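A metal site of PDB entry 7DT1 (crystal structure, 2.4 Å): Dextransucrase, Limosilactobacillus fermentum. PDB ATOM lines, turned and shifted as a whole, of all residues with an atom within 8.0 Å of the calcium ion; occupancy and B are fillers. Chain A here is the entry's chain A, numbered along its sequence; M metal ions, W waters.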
ATOM      1  N   MET A 379       8.669 -34.266  19.002  1.00  0.00           N
ATOM      2  CA  MET A 379       8.672 -32.811  19.067  1.00  0.00           C
ATOM      3  C   MET A 379       7.702 -32.238  18.055  1.00  0.00           C
ATOM      4  O   MET A 379       7.402 -32.863  17.036  1.00  0.00           O
ATOM      5  CB  MET A 379      10.083 -32.264  18.847  1.00  0.00           C
ATOM      6  CG  MET A 379      11.063 -32.839  19.842  1.00  0.00           C
ATOM      7  SD  MET A 379      12.760 -32.250  19.725  1.00  0.00           S
ATOM      8  CE  MET A 379      13.205 -32.970  18.152  1.00  0.00           C
ATOM      9  N   ASN A 380       7.172 -31.065  18.391  1.00  0.00           N
ATOM     10  CA  ASN A 380       6.222 -30.297  17.575  1.00  0.00           C
ATOM     11  C   ASN A 380       4.867 -30.969  17.483  1.00  0.00           C
ATOM     12  O   ASN A 380       4.118 -30.707  16.534  1.00  0.00           O
ATOM     13  CB  ASN A 380       6.784 -30.008  16.178  1.00  0.00           C
ATOM     14  CG  ASN A 380       8.065 -29.185  16.231  1.00  0.00           C
ATOM     15  OD1 ASN A 380       8.087 -28.100  16.796  1.00  0.00           O
ATOM     16  ND2 ASN A 380       9.156 -29.733  15.691  1.00  0.00           N
ATOM     17  N   THR A 382       2.335 -30.068  18.791  1.00  0.00           N
ATOM     18  CA  THR A 382       1.816 -28.864  19.420  1.00  0.00           C
ATOM     19  C   THR A 382       0.507 -28.454  18.766  1.00  0.00           C
ATOM     20  O   THR A 382       0.386 -28.508  17.536  1.00  0.00           O
ATOM     21  CB  THR A 382       2.851 -27.763  19.259  1.00  0.00           C
ATOM     22  OG1 THR A 382       3.147 -27.597  17.861  1.00  0.00           O
ATOM     23  CG2 THR A 382       4.128 -28.157  19.974  1.00  0.00           C
ATOM     24  N   PRO A 396       6.444 -23.922  17.421  1.00  0.00           N
ATOM     25  CA  PRO A 396       7.713 -24.604  17.702  1.00  0.00           C
ATOM     26  C   PRO A 396       7.755 -25.234  19.076  1.00  0.00           C
ATOM     27  O   PRO A 396       7.118 -24.757  20.030  1.00  0.00           O
ATOM     28  CB  PRO A 396       8.748 -23.476  17.584  1.00  0.00           C
ATOM     29  CG  PRO A 396       8.004 -22.283  18.084  1.00  0.00           C
ATOM     30  CD  PRO A 396       6.577 -22.461  17.573  1.00  0.00           C
ATOM     31  N   GLU A 397       8.561 -26.286  19.166  1.00  0.00           N
ATOM     32  CA  GLU A 397       8.725 -27.042  20.406  1.00  0.00           C
ATOM     33  C   GLU A 397       9.696 -26.367  21.391  1.00  0.00           C
ATOM     34  O   GLU A 397       9.507 -26.489  22.601  1.00  0.00           O
ATOM     35  CB  GLU A 397       9.238 -28.440  20.065  1.00  0.00           C
ATOM     36  CG  GLU A 397       9.543 -29.302  21.284  1.00  0.00           C
ATOM     37  CD  GLU A 397       8.290 -29.677  22.031  1.00  0.00           C
ATOM     38  OE1 GLU A 397       7.526 -30.514  21.501  1.00  0.00           O
ATOM     39  OE2 GLU A 397       8.049 -29.138  23.139  1.00  0.00           O
ATOM     40  N   LEU A 398      10.721 -25.669  20.902  1.00  0.00           N
ATOM     41  CA  LEU A 398      11.809 -25.206  21.749  1.00  0.00           C
ATOM     42  C   LEU A 398      11.709 -23.688  21.944  1.00  0.00           C
ATOM     43  O   LEU A 398      11.530 -22.943  20.977  1.00  0.00           O
ATOM     44  CB  LEU A 398      13.161 -25.597  21.144  1.00  0.00           C
ATOM     45  CG  LEU A 398      13.281 -27.104  20.808  1.00  0.00           C
ATOM     46  CD1 LEU A 398      14.363 -27.390  19.799  1.00  0.00           C
ATOM     47  CD2 LEU A 398      13.513 -27.947  22.052  1.00  0.00           C
ATOM     48  N   LEU A 399      11.782 -23.238  23.201  1.00  0.00           N
ATOM     49  CA  LEU A 399      11.815 -21.821  23.510  1.00  0.00           C
ATOM     50  C   LEU A 399      13.135 -21.448  24.166  1.00  0.00           C
ATOM     51  O   LEU A 399      13.987 -20.847  23.518  1.00  0.00           O
ATOM     52  CB  LEU A 399      10.627 -21.433  24.385  1.00  0.00           C
ATOM     53  CG  LEU A 399       9.194 -21.670  23.914  1.00  0.00           C
ATOM     54  CD1 LEU A 399       8.207 -21.296  25.014  1.00  0.00           C
ATOM     55  CD2 LEU A 399       8.858 -20.917  22.632  1.00  0.00           C
ATOM     56  N   VAL A 400      13.347 -21.807  25.431  1.00  0.00           N
ATOM     57  CA  VAL A 400      14.567 -21.440  26.134  1.00  0.00           C
ATOM     58  C   VAL A 400      14.768 -22.429  27.261  1.00  0.00           C
ATOM     59  O   VAL A 400      13.797 -22.951  27.818  1.00  0.00           O
ATOM     60  CB  VAL A 400      14.498 -19.971  26.644  1.00  0.00           C
ATOM     61  CG1 VAL A 400      13.249 -19.775  27.509  1.00  0.00           C
ATOM     62  CG2 VAL A 400      15.762 -19.614  27.433  1.00  0.00           C
ATOM     63  N   ASN A 402      16.185 -25.928  29.332  1.00  0.00           N
ATOM     64  CA  ASN A 402      16.077 -27.372  29.135  1.00  0.00           C
ATOM     65  C   ASN A 402      14.630 -27.713  28.819  1.00  0.00           C
ATOM     66  O   ASN A 402      13.778 -27.784  29.717  1.00  0.00           O
ATOM     67  CB  ASN A 402      16.545 -28.124  30.377  1.00  0.00           C
ATOM     68  CG  ASN A 402      18.025 -28.025  30.579  1.00  0.00           C
ATOM     69  OD1 ASN A 402      18.550 -26.944  30.797  1.00  0.00           O
ATOM     70  ND2 ASN A 402      18.695 -29.157  30.506  1.00  0.00           N
ATOM     71  N   ASP A 403      14.357 -27.969  27.549  1.00  0.00           N
ATOM     72  CA  ASP A 403      13.012 -28.308  27.119  1.00  0.00           C
ATOM     73  C   ASP A 403      12.666 -29.725  27.571  1.00  0.00           C
ATOM     74  O   ASP A 403      13.408 -30.676  27.320  1.00  0.00           O
ATOM     75  CB  ASP A 403      12.901 -28.181  25.605  1.00  0.00           C
ATOM     76  CG  ASP A 403      11.466 -28.097  25.150  1.00  0.00           C
ATOM     77  OD1 ASP A 403      10.844 -27.041  25.365  1.00  0.00           O
ATOM     78  OD2 ASP A 403      10.951 -29.079  24.598  1.00  0.00           O
ATOM     79  N   ILE A 404      11.501 -29.868  28.201  1.00  0.00           N
ATOM     80  CA  ILE A 404      11.078 -31.124  28.786  1.00  0.00           C
ATOM     81  C   ILE A 404      10.350 -31.945  27.728  1.00  0.00           C
ATOM     82  O   ILE A 404       9.496 -31.423  27.000  1.00  0.00           O
ATOM     83  CB  ILE A 404      10.178 -30.885  30.000  1.00  0.00           C
ATOM     84  CG1 ILE A 404      10.934 -30.065  31.052  1.00  0.00           C
ATOM     85  CG2 ILE A 404       9.723 -32.206  30.598  1.00  0.00           C
ATOM     86  CD1 ILE A 404      12.316 -30.612  31.417  1.00  0.00           C
ATOM     87  N   ASP A 405      10.670 -33.235  27.634  1.00  0.00           N
ATOM     88  CA  ASP A 405      10.025 -34.082  26.650  1.00  0.00           C
ATOM     89  C   ASP A 405       8.676 -34.509  27.219  1.00  0.00           C
ATOM     90  O   ASP A 405       8.524 -35.573  27.835  1.00  0.00           O
ATOM     91  CB  ASP A 405      10.902 -35.279  26.288  1.00  0.00           C
ATOM     92  CG  ASP A 405      10.191 -36.259  25.353  1.00  0.00           C
ATOM     93  OD1 ASP A 405       9.160 -35.884  24.749  1.00  0.00           O
ATOM     94  OD2 ASP A 405      10.663 -37.406  25.248  1.00  0.00           O
ATOM     95  N   ASN A 406       7.666 -33.667  27.001  1.00  0.00           N
ATOM     96  CA  ASN A 406       6.305 -33.948  27.451  1.00  0.00           C
ATOM     97  C   ASN A 406       5.620 -35.034  26.626  1.00  0.00           C
ATOM     98  O   ASN A 406       4.428 -35.282  26.845  1.00  0.00           O
ATOM     99  CB  ASN A 406       5.475 -32.663  27.434  1.00  0.00           C
ATOM    100  CG  ASN A 406       5.818 -31.758  28.605  1.00  0.00           C
ATOM    101  OD1 ASN A 406       5.745 -32.169  29.756  1.00  0.00           O
ATOM    102  ND2 ASN A 406       6.226 -30.525  28.306  1.00  0.00           N
ATOM    103  N   ALA A 444       2.883 -21.681  27.982  1.00  0.00           N
ATOM    104  CA  ALA A 444       3.510 -22.194  26.770  1.00  0.00           C
ATOM    105  C   ALA A 444       2.797 -23.450  26.288  1.00  0.00           C
ATOM    106  O   ALA A 444       3.417 -24.432  25.876  1.00  0.00           O
ATOM    107  CB  ALA A 444       5.010 -22.450  26.981  1.00  0.00           C
ATOM    108  N   ASP A 446       1.256 -23.678  23.654  1.00  0.00           N
ATOM    109  CA  ASP A 446       1.548 -23.829  22.236  1.00  0.00           C
ATOM    110  C   ASP A 446       2.866 -24.546  21.990  1.00  0.00           C
ATOM    111  O   ASP A 446       3.202 -24.787  20.829  1.00  0.00           O
ATOM    112  CB  ASP A 446       1.591 -22.459  21.542  1.00  0.00           C
ATOM    113  CG  ASP A 446       0.210 -21.825  21.412  1.00  0.00           C
ATOM    114  OD1 ASP A 446      -0.796 -22.451  21.810  1.00  0.00           O
ATOM    115  OD2 ASP A 446       0.155 -20.680  20.898  1.00  0.00           O
ATOM    116  N   ASN A 447       3.590 -24.899  23.040  1.00  0.00           N
ATOM    117  CA  ASN A 447       4.974 -25.348  22.881  1.00  0.00           C
ATOM    118  C   ASN A 447       5.248 -26.675  23.569  1.00  0.00           C
ATOM    119  O   ASN A 447       6.389 -27.135  23.572  1.00  0.00           O
ATOM    120  CB  ASN A 447       5.904 -24.250  23.382  1.00  0.00           C
ATOM    121  CG  ASN A 447       5.606 -22.949  22.707  1.00  0.00           C
ATOM    122  OD1 ASN A 447       4.985 -22.092  23.297  1.00  0.00           O
ATOM    123  ND2 ASN A 447       5.950 -22.843  21.427  1.00  0.00           N
ATOM    124  N   ILE A 448       4.235 -27.308  24.115  1.00  0.00           N
ATOM    125  CA  ILE A 448       4.410 -28.602  24.741  1.00  0.00           C
ATOM    126  C   ILE A 448       3.580 -29.604  23.949  1.00  0.00           C
ATOM    127  O   ILE A 448       2.655 -29.234  23.198  1.00  0.00           O
ATOM    128  CB  ILE A 448       4.001 -28.553  26.232  1.00  0.00           C
ATOM    129  CG1 ILE A 448       2.576 -28.015  26.368  1.00  0.00           C
ATOM    130  CG2 ILE A 448       5.005 -27.655  27.034  1.00  0.00           C
ATOM    131  CD1 ILE A 448       2.199 -27.581  27.795  1.00  0.00           C
ATOM    132  N   ASP A 449       3.962 -30.871  24.039  1.00  0.00           N
ATOM    133  CA  ASP A 449       3.106 -31.905  23.481  1.00  0.00           C
ATOM    134  C   ASP A 449       1.687 -31.707  24.024  1.00  0.00           C
ATOM    135  O   ASP A 449       1.491 -31.582  25.234  1.00  0.00           O
ATOM    136  CB  ASP A 449       3.652 -33.278  23.856  1.00  0.00           C
ATOM    137  CG  ASP A 449       2.908 -34.427  23.190  1.00  0.00           C
ATOM    138  OD1 ASP A 449       1.664 -34.403  23.076  1.00  0.00           O
ATOM    139  OD2 ASP A 449       3.603 -35.381  22.808  1.00  0.00           O
ATOM    140  N   MET A 904       5.094 -26.419  32.235  1.00  0.00           N
ATOM    141  CA  MET A 904       5.610 -27.718  31.814  1.00  0.00           C
ATOM    142  C   MET A 904       6.660 -27.643  30.717  1.00  0.00           C
ATOM    143  O   MET A 904       7.215 -28.681  30.356  1.00  0.00           O
ATOM    144  CB  MET A 904       4.467 -28.612  31.349  1.00  0.00           C
ATOM    145  CG  MET A 904       3.764 -29.314  32.529  1.00  0.00           C
ATOM    146  SD  MET A 904       2.267 -30.148  32.013  1.00  0.00           S
ATOM    147  CE  MET A 904       1.123 -28.784  31.918  1.00  0.00           C
ATOM    148  N   ASN A 905       6.963 -26.453  30.199  1.00  0.00           N
ATOM    149  CA  ASN A 905       7.804 -26.425  29.020  1.00  0.00           C
ATOM    150  C   ASN A 905       9.265 -26.666  29.323  1.00  0.00           C
ATOM    151  O   ASN A 905       9.932 -27.375  28.567  1.00  0.00           O
ATOM    152  CB  ASN A 905       7.668 -25.119  28.265  1.00  0.00           C
ATOM    153  CG  ASN A 905       8.500 -25.141  26.995  1.00  0.00           C
ATOM    154  OD1 ASN A 905       8.161 -25.869  26.048  1.00  0.00           O
ATOM    155  ND2 ASN A 905       9.625 -24.404  26.991  1.00  0.00           N
ATOM    156  N   GLN A 906       9.807 -26.059  30.381  1.00  0.00           N
ATOM    157  CA  GLN A 906      11.259 -26.107  30.538  1.00  0.00           C
ATOM    158  C   GLN A 906      11.664 -25.850  31.990  1.00  0.00           C
ATOM    159  O   GLN A 906      10.941 -25.206  32.757  1.00  0.00           O
ATOM    160  CB  GLN A 906      11.968 -25.080  29.624  1.00  0.00           C
ATOM    161  CG  GLN A 906      12.006 -23.658  30.192  1.00  0.00           C
ATOM    162  CD  GLN A 906      10.651 -22.963  30.092  1.00  0.00           C
ATOM    163  OE1 GLN A 906      10.013 -22.979  29.021  1.00  0.00           O
ATOM    164  NE2 GLN A 906      10.194 -22.368  31.196  1.00  0.00           N
ATOM    165  N   GLY A 923      14.199 -23.220  16.548  1.00  0.00           N
ATOM    166  CA  GLY A 923      13.138 -23.428  17.527  1.00  0.00           C
ATOM    167  C   GLY A 923      12.223 -24.605  17.219  1.00  0.00           C
ATOM    168  O   GLY A 923      11.577 -25.130  18.142  1.00  0.00           O
ATOM    169  N   ASN A 996      13.961 -32.924  25.594  1.00  0.00           N
ATOM    170  CA  ASN A 996      14.117 -32.862  24.139  1.00  0.00           C
ATOM    171  C   ASN A 996      15.429 -32.229  23.721  1.00  0.00           C
ATOM    172  O   ASN A 996      15.972 -32.583  22.673  1.00  0.00           O
ATOM    173  CB  ASN A 996      12.971 -32.073  23.498  1.00  0.00           C
ATOM    174  CG  ASN A 996      11.653 -32.804  23.540  1.00  0.00           C
ATOM    175  OD1 ASN A 996      11.606 -34.023  23.361  1.00  0.00           O
ATOM    176  ND2 ASN A 996      10.562 -32.059  23.787  1.00  0.00           N
HETATM  177 CA    CA M   1       8.713 -27.658  24.532  1.00  0.00          CA
HETATM  178  O   HOH W   1       8.668 -28.977  26.559  1.00  0.00           O
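N of Glu 397 sits at hydrogen-bond distance from OD1 of Asn 380 (3.0 Å).
O of Gly 923 is in hydrogen-bond range of N of Glu 397 (3.4 Å).
The backbone carbonyl oxygen (O) of Asp 403 lies within hydrogen-bond range of the backbone NH (N) of Asn 996, 2.9 Å away.
The backbone NH (N) of Ile 404 lies within hydrogen-bond range of the backbone carbonyl oxygen (O) of Asn 905.
ND2 of Asn 905 is in hydrogen-bond range of OE1 of Gln 906 (2.5 Å).
ND2 of Asn 447 sits at hydrogen-bond distance from O of Pro 396, at 2.6 Å.
The calcium ion is bound by the side-chain carboxylate (OE2) of Glu 397 (2.1 Å), the side-chain carboxylate (OD1) of Asp 403 (2.4 Å), the backbone carbonyl oxygen (O) of Glu 397 (2.4 Å), the side-chain amide oxygen (OD1) of Asn 905 (2.4 Å), water W1 (2.4 Å), the backbone carbonyl oxygen (O) of Asn 447 (2.6 Å) and the side-chain carboxylate (OD2) of Asp 403 (2.7 Å).
Water W1 lies within hydrogen-bond range of O of Ile 404 (2.6 Å), O of Asn 905 (2.9 Å) and ND2 of Asn 406 (3.4 Å).
Of the 23 residues printed, 4 come within 4 Å of the calcium ion.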
